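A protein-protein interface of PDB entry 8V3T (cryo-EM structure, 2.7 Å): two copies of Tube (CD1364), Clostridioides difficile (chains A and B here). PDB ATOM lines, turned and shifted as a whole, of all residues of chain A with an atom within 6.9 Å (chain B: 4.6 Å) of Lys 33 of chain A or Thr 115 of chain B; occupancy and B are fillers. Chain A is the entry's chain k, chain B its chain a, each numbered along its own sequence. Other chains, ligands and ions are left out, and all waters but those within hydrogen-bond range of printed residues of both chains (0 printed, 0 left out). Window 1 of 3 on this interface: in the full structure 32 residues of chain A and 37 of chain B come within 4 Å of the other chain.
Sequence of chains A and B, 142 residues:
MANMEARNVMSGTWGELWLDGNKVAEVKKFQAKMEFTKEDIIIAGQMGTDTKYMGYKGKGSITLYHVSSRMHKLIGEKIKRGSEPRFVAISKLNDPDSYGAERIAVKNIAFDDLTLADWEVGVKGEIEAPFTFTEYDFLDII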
ATOM      1  N   GLN A  31      21.330 -15.539  14.832  1.00  0.00           N
ATOM      2  CA  GLN A  31      20.470 -14.640  14.078  1.00  0.00           C
ATOM      3  C   GLN A  31      19.377 -15.434  13.376  1.00  0.00           C
ATOM      4  O   GLN A  31      19.626 -16.527  12.864  1.00  0.00           O
ATOM      5  CB  GLN A  31      21.283 -13.845  13.054  1.00  0.00           C
ATOM      6  CG  GLN A  31      21.395 -12.371  13.366  1.00  0.00           C
ATOM      7  CD  GLN A  31      21.953 -11.576  12.206  1.00  0.00           C
ATOM      8  OE1 GLN A  31      23.167 -11.439  12.060  1.00  0.00           O
ATOM      9  NE2 GLN A  31      21.068 -11.052  11.367  1.00  0.00           N
ATOM     10  N   ALA A  32      18.173 -14.868  13.353  1.00  0.00           N
ATOM     11  CA  ALA A  32      17.042 -15.468  12.655  1.00  0.00           C
ATOM     12  C   ALA A  32      16.037 -14.370  12.346  1.00  0.00           C
ATOM     13  O   ALA A  32      15.700 -13.578  13.229  1.00  0.00           O
ATOM     14  CB  ALA A  32      16.396 -16.575  13.493  1.00  0.00           C
ATOM     15  N   LYS A  33      15.556 -14.329  11.106  1.00  0.00           N
ATOM     16  CA  LYS A  33      14.715 -13.223  10.670  1.00  0.00           C
ATOM     17  C   LYS A  33      13.867 -13.668   9.487  1.00  0.00           C
ATOM     18  O   LYS A  33      14.298 -14.484   8.670  1.00  0.00           O
ATOM     19  CB  LYS A  33      15.574 -12.009  10.300  1.00  0.00           C
ATOM     20  CG  LYS A  33      14.810 -10.805   9.794  1.00  0.00           C
ATOM     21  CD  LYS A  33      15.679  -9.974   8.871  1.00  0.00           C
ATOM     22  CE  LYS A  33      15.631  -8.504   9.230  1.00  0.00           C
ATOM     23  NZ  LYS A  33      16.401  -8.226  10.471  1.00  0.00           N
ATOM     24  N   MET A  34      12.659 -13.114   9.401  1.00  0.00           N
ATOM     25  CA  MET A  34      11.713 -13.426   8.337  1.00  0.00           C
ATOM     26  C   MET A  34      11.522 -12.208   7.443  1.00  0.00           C
ATOM     27  O   MET A  34      11.165 -11.134   7.930  1.00  0.00           O
ATOM     28  CB  MET A  34      10.366 -13.860   8.915  1.00  0.00           C
ATOM     29  CG  MET A  34      10.330 -15.290   9.408  1.00  0.00           C
ATOM     30  SD  MET A  34       9.301 -15.472  10.874  1.00  0.00           S
ATOM     31  CE  MET A  34       7.671 -15.266  10.165  1.00  0.00           C
ATOM     32  N   GLU A  35      11.736 -12.382   6.139  1.00  0.00           N
ATOM     33  CA  GLU A  35      11.597 -11.313   5.155  1.00  0.00           C
ATOM     34  C   GLU A  35      10.312 -11.523   4.369  1.00  0.00           C
ATOM     35  O   GLU A  35      10.134 -12.574   3.747  1.00  0.00           O
ATOM     36  CB  GLU A  35      12.785 -11.287   4.192  1.00  0.00           C
ATOM     37  CG  GLU A  35      14.110 -11.716   4.778  1.00  0.00           C
ATOM     38  CD  GLU A  35      14.894 -10.557   5.345  1.00  0.00           C
ATOM     39  OE1 GLU A  35      14.430  -9.405   5.215  1.00  0.00           O
ATOM     40  OE2 GLU A  35      15.988 -10.795   5.895  1.00  0.00           O
ATOM     41  N   TYR A  56       6.916 -15.236   2.833  1.00  0.00           N
ATOM     42  CA  TYR A  56       8.098 -14.820   3.579  1.00  0.00           C
ATOM     43  C   TYR A  56       9.285 -15.756   3.356  1.00  0.00           C
ATOM     44  O   TYR A  56       9.141 -16.911   2.949  1.00  0.00           O
ATOM     45  CB  TYR A  56       7.793 -14.690   5.081  1.00  0.00           C
ATOM     46  CG  TYR A  56       7.533 -15.985   5.817  1.00  0.00           C
ATOM     47  CD1 TYR A  56       8.580 -16.742   6.319  1.00  0.00           C
ATOM     48  CD2 TYR A  56       6.238 -16.435   6.037  1.00  0.00           C
ATOM     49  CE1 TYR A  56       8.351 -17.919   6.997  1.00  0.00           C
ATOM     50  CE2 TYR A  56       5.998 -17.611   6.717  1.00  0.00           C
ATOM     51  CZ  TYR A  56       7.057 -18.349   7.194  1.00  0.00           C
ATOM     52  OH  TYR A  56       6.811 -19.519   7.870  1.00  0.00           O
ATOM     53  N   LYS A  57      10.465 -15.213   3.658  1.00  0.00           N
ATOM     54  CA  LYS A  57      11.765 -15.882   3.690  1.00  0.00           C
ATOM     55  C   LYS A  57      12.364 -15.830   5.083  1.00  0.00           C
ATOM     56  O   LYS A  57      12.482 -14.751   5.667  1.00  0.00           O
ATOM     57  CB  LYS A  57      12.740 -15.225   2.713  1.00  0.00           C
ATOM     58  CG  LYS A  57      12.523 -15.535   1.275  1.00  0.00           C
ATOM     59  CD  LYS A  57      12.927 -16.989   1.142  1.00  0.00           C
ATOM     60  CE  LYS A  57      12.224 -17.778   0.093  1.00  0.00           C
ATOM     61  NZ  LYS A  57      12.070 -19.123   0.704  1.00  0.00           N
ATOM     62  N   GLY A  58      12.774 -16.985   5.593  1.00  0.00           N
ATOM     63  CA  GLY A  58      13.556 -17.054   6.814  1.00  0.00           C
ATOM     64  C   GLY A  58      15.034 -17.187   6.489  1.00  0.00           C
ATOM     65  O   GLY A  58      15.434 -18.065   5.725  1.00  0.00           O
ATOM     66  N   LYS A  59      15.839 -16.310   7.085  1.00  0.00           N
ATOM     67  CA  LYS A  59      17.280 -16.307   6.888  1.00  0.00           C
ATOM     68  C   LYS A  59      17.969 -16.050   8.219  1.00  0.00           C
ATOM     69  O   LYS A  59      17.475 -15.287   9.052  1.00  0.00           O
ATOM     70  CB  LYS A  59      17.716 -15.248   5.868  1.00  0.00           C
ATOM     71  CG  LYS A  59      17.237 -15.517   4.456  1.00  0.00           C
ATOM     72  CD  LYS A  59      16.711 -14.253   3.806  1.00  0.00           C
ATOM     73  CE  LYS A  59      17.522 -13.877   2.581  1.00  0.00           C
ATOM     74  NZ  LYS A  59      16.653 -13.343   1.495  1.00  0.00           N
ATOM     75  N   GLY A  60      19.122 -16.684   8.406  1.00  0.00           N
ATOM     76  CA  GLY A  60      19.865 -16.528   9.641  1.00  0.00           C
ATOM     77  C   GLY A  60      21.317 -16.896   9.439  1.00  0.00           C
ATOM     78  O   GLY A  60      21.752 -17.225   8.334  1.00  0.00           O
ATOM     79  N   GLU A 102      13.568 -15.221  26.833  1.00  0.00           N
ATOM     80  CA  GLU A 102      13.032 -15.359  25.485  1.00  0.00           C
ATOM     81  C   GLU A 102      13.640 -16.607  24.861  1.00  0.00           C
ATOM     82  O   GLU A 102      14.860 -16.680  24.689  1.00  0.00           O
ATOM     83  CB  GLU A 102      13.344 -14.123  24.638  1.00  0.00           C
ATOM     84  CG  GLU A 102      12.496 -13.988  23.388  1.00  0.00           C
ATOM     85  CD  GLU A 102      12.483 -12.572  22.843  1.00  0.00           C
ATOM     86  OE1 GLU A 102      11.659 -11.760  23.310  1.00  0.00           O
ATOM     87  OE2 GLU A 102      13.298 -12.272  21.946  1.00  0.00           O
ATOM     88  N   ILE A 104      13.193 -19.426  21.654  1.00  0.00           N
ATOM     89  CA  ILE A 104      12.579 -19.676  20.358  1.00  0.00           C
ATOM     90  C   ILE A 104      13.217 -20.908  19.734  1.00  0.00           C
ATOM     91  O   ILE A 104      14.438 -21.087  19.797  1.00  0.00           O
ATOM     92  CB  ILE A 104      12.712 -18.458  19.419  1.00  0.00           C
ATOM     93  CG1 ILE A 104      12.227 -17.188  20.117  1.00  0.00           C
ATOM     94  CG2 ILE A 104      11.939 -18.679  18.130  1.00  0.00           C
ATOM     95  CD1 ILE A 104      12.324 -15.955  19.268  1.00  0.00           C
ATOM     96  N   PHE A 131      22.269 -19.837   7.019  1.00  0.00           N
ATOM     97  CA  PHE A 131      21.275 -20.881   6.808  1.00  0.00           C
ATOM     98  C   PHE A 131      19.942 -20.241   6.447  1.00  0.00           C
ATOM     99  O   PHE A 131      19.776 -19.021   6.506  1.00  0.00           O
ATOM    100  CB  PHE A 131      21.136 -21.782   8.044  1.00  0.00           C
ATOM    101  CG  PHE A 131      20.656 -21.067   9.278  1.00  0.00           C
ATOM    102  CD1 PHE A 131      19.303 -20.872   9.507  1.00  0.00           C
ATOM    103  CD2 PHE A 131      21.558 -20.598  10.215  1.00  0.00           C
ATOM    104  CE1 PHE A 131      18.863 -20.219  10.641  1.00  0.00           C
ATOM    105  CE2 PHE A 131      21.124 -19.944  11.349  1.00  0.00           C
ATOM    106  CZ  PHE A 131      19.776 -19.755  11.562  1.00  0.00           C
ATOM    107  N   PHE A 133      15.449 -21.227   6.817  1.00  0.00           N
ATOM    108  CA  PHE A 133      14.505 -21.983   7.633  1.00  0.00           C
ATOM    109  C   PHE A 133      13.086 -21.648   7.196  1.00  0.00           C
ATOM    110  O   PHE A 133      12.854 -20.718   6.422  1.00  0.00           O
ATOM    111  CB  PHE A 133      14.710 -21.706   9.126  1.00  0.00           C
ATOM    112  CG  PHE A 133      14.297 -20.328   9.557  1.00  0.00           C
ATOM    113  CD1 PHE A 133      15.181 -19.267   9.468  1.00  0.00           C
ATOM    114  CD2 PHE A 133      13.030 -20.092  10.063  1.00  0.00           C
ATOM    115  CE1 PHE A 133      14.810 -18.002   9.869  1.00  0.00           C
ATOM    116  CE2 PHE A 133      12.652 -18.828  10.461  1.00  0.00           C
ATOM    117  CZ  PHE A 133      13.543 -17.783  10.362  1.00  0.00           C
ATOM    118  N   HIS B  72       6.851  -9.516  18.080  1.00  0.00           N
ATOM    119  CA  HIS B  72       6.402 -10.904  18.050  1.00  0.00           C
ATOM    120  C   HIS B  72       4.912 -10.985  18.346  1.00  0.00           C
ATOM    121  O   HIS B  72       4.131 -11.485  17.529  1.00  0.00           O
ATOM    122  CB  HIS B  72       7.185 -11.748  19.061  1.00  0.00           C
ATOM    123  CG  HIS B  72       8.672 -11.571  19.000  1.00  0.00           C
ATOM    124  ND1 HIS B  72       9.294 -10.368  19.251  1.00  0.00           N
ATOM    125  CD2 HIS B  72       9.662 -12.455  18.732  1.00  0.00           C
ATOM    126  CE1 HIS B  72      10.601 -10.516  19.134  1.00  0.00           C
ATOM    127  NE2 HIS B  72      10.851 -11.773  18.819  1.00  0.00           N
ATOM    128  N   ASP B 113       9.339  -6.862   7.854  1.00  0.00           N
ATOM    129  CA  ASP B 113       9.950  -8.109   8.296  1.00  0.00           C
ATOM    130  C   ASP B 113       9.675  -8.300   9.782  1.00  0.00           C
ATOM    131  O   ASP B 113       9.068  -7.450  10.439  1.00  0.00           O
ATOM    132  CB  ASP B 113      11.452  -8.122   7.990  1.00  0.00           C
ATOM    133  CG  ASP B 113      12.205  -7.006   8.684  1.00  0.00           C
ATOM    134  OD1 ASP B 113      12.333  -7.045   9.926  1.00  0.00           O
ATOM    135  OD2 ASP B 113      12.678  -6.088   7.985  1.00  0.00           O
ATOM    136  N   LEU B 114      10.129  -9.436  10.308  1.00  0.00           N
ATOM    137  CA  LEU B 114      10.018  -9.755  11.724  1.00  0.00           C
ATOM    138  C   LEU B 114      11.324 -10.374  12.192  1.00  0.00           C
ATOM    139  O   LEU B 114      11.817 -11.322  11.576  1.00  0.00           O
ATOM    140  CB  LEU B 114       8.852 -10.714  11.993  1.00  0.00           C
ATOM    141  CG  LEU B 114       8.752 -11.268  13.416  1.00  0.00           C
ATOM    142  CD1 LEU B 114       8.605 -10.143  14.424  1.00  0.00           C
ATOM    143  CD2 LEU B 114       7.600 -12.249  13.534  1.00  0.00           C
ATOM    144  N   THR B 115      11.874  -9.845  13.280  1.00  0.00           N
ATOM    145  CA  THR B 115      13.132 -10.324  13.837  1.00  0.00           C
ATOM    146  C   THR B 115      12.837 -11.228  15.025  1.00  0.00           C
ATOM    147  O   THR B 115      12.216 -10.794  16.001  1.00  0.00           O
ATOM    148  CB  THR B 115      14.021  -9.156  14.264  1.00  0.00           C
ATOM    149  OG1 THR B 115      14.323  -8.341  13.127  1.00  0.00           O
ATOM    150  CG2 THR B 115      15.314  -9.665  14.871  1.00  0.00           C
ATOM    151  N   LEU B 116      13.281 -12.482  14.942  1.00  0.00           N
ATOM    152  CA  LEU B 116      13.066 -13.437  16.021  1.00  0.00           C
ATOM    153  C   LEU B 116      14.214 -13.433  17.025  1.00  0.00           C
ATOM    154  O   LEU B 116      13.980 -13.404  18.235  1.00  0.00           O
ATOM    155  CB  LEU B 116      12.870 -14.845  15.451  1.00  0.00           C
ATOM    156  CG  LEU B 116      11.838 -15.008  14.336  1.00  0.00           C
ATOM    157  CD1 LEU B 116      11.840 -16.432  13.816  1.00  0.00           C
ATOM    158  CD2 LEU B 116      10.454 -14.617  14.823  1.00  0.00           C
ATOM    159  N   ALA B 117      15.454 -13.458  16.543  1.00  0.00           N
ATOM    160  CA  ALA B 117      16.608 -13.458  17.428  1.00  0.00           C
ATOM    161  C   ALA B 117      17.774 -12.769  16.739  1.00  0.00           C
ATOM    162  O   ALA B 117      18.057 -13.034  15.568  1.00  0.00           O
ATOM    163  CB  ALA B 117      17.006 -14.880  17.833  1.00  0.00           C
ATOM    164  N   ASP B 118      18.434 -11.869  17.471  1.00  0.00           N
ATOM    165  CA  ASP B 118      19.654 -11.230  16.984  1.00  0.00           C
ATOM    166  C   ASP B 118      20.446 -10.781  18.211  1.00  0.00           C
ATOM    167  O   ASP B 118      20.132  -9.746  18.802  1.00  0.00           O
ATOM    168  CB  ASP B 118      19.329 -10.063  16.066  1.00  0.00           C
ATOM    169  CG  ASP B 118      20.542  -9.555  15.313  1.00  0.00           C
ATOM    170  OD1 ASP B 118      21.661 -10.045  15.573  1.00  0.00           O
ATOM    171  OD2 ASP B 118      20.376  -8.659  14.459  1.00  0.00           O
ATOM    172  N   GLU B 128      15.478  -3.224  14.627  1.00  0.00           N
ATOM    173  CA  GLU B 128      15.140  -2.279  13.570  1.00  0.00           C
ATOM    174  C   GLU B 128      13.997  -2.850  12.741  1.00  0.00           C
ATOM    175  O   GLU B 128      14.077  -3.988  12.273  1.00  0.00           O
ATOM    176  CB  GLU B 128      16.356  -1.995  12.687  1.00  0.00           C
ATOM    177  CG  GLU B 128      16.028  -1.295  11.386  1.00  0.00           C
ATOM    178  CD  GLU B 128      17.135  -0.365  10.938  1.00  0.00           C
ATOM    179  OE1 GLU B 128      17.910   0.094  11.802  1.00  0.00           O
ATOM    180  OE2 GLU B 128      17.233  -0.096   9.722  1.00  0.00           O
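No position is printed for both chains.
Of the 11 pairs that touch across the chains among the printed residues, none has its exchanged pair printed and touching as well.
Among the printed residues, merely in contact across the chains: Gln 31 of chain A with Ala 117 of chain B, Gln 31 of chain A with Asp 118 of chain B, Lys 33 of chain A with Asp 113 of chain B, Lys 33 of chain A with Leu 114 of chain B, Met 34 of chain A with Asp 113 of chain B, Glu 102 of chain A with Leu 116 of chain B and Ile 104 of chain A with Leu 116 of chain B.
Of the 8 printed residues of chain B, 6 touch a printed residue of chain A.
Hydrophobic or aromatic side chains of chain B within 4 Å of the printed part of chain A: Leu 116.
Of the 14 printed residues of chain A, 6 touch a printed residue of chain B.
Hydrophobic or aromatic side chains of chain A within 4 Å of the printed part of chain B: Met 34 and Ile 104.
Among the printed residues, 11 pairs touch across the chains.
Among the printed residues, no Asp or Glu carboxylate lies within 4 Å of a Lys or Arg side-chain nitrogen of the other chain.
NE2 of His 72 of chain B sits at hydrogen-bond distance from O of Thr 115 of chain B (3.3 Å).
N of Lys 59 of chain A is in hydrogen-bond range of O of Lys 33 of chain A (2.9 Å).
Lys 33 of chain A touches three residues of chain B.
Thr 115 of chain B touches just one residue of chain A: Lys 33 (3.4 Å).
Of the printed residues of chain A, Ala 117 of chain B touches Gln 31 and Ala 32.
Of the printed residues of chain B, Gln 31 of chain A touches Ala 117 and Asp 118.
Printed residues of chain B within 4 Å of Glu 102 of chain A: Leu 116.
Printed residues of chain B within 4 Å of Met 34 of chain A: Asp 113 (3.0 Å) and Leu 114 (2.9 Å).
Of the printed residues of chain A, Asp 113 of chain B touches Lys 33 and Met 34.
Gly 58 of chain A touches none of the printed residues of chain B.
The nearest printed residue of chain B that does not touch Lys 33 of chain A is Leu 116 of chain B (4.6 Å).
The nearest residue of chain A that does not touch Thr 115 of chain B is Ala 32 of chain A (4.1 Å).
The backbone NH (N) of Met 34 of chain A is in hydrogen-bond range of the backbone carbonyl oxygen (O) of Leu 114 of chain B, 2.9 Å away.
NZ of Lys 33 of chain A sits at hydrogen-bond distance from OG1 of Thr 115 of chain B (3.4 Å).
The backbone carbonyl oxygen (O) of Ala 32 of chain A is in hydrogen-bond range of the backbone NH (N) of Leu 116 of chain B (3.2 Å).
The backbone NH (N) of Ala 32 of chain A sits at hydrogen-bond distance from the backbone carbonyl oxygen (O) of Ala 117 of chain B (2.9 Å).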
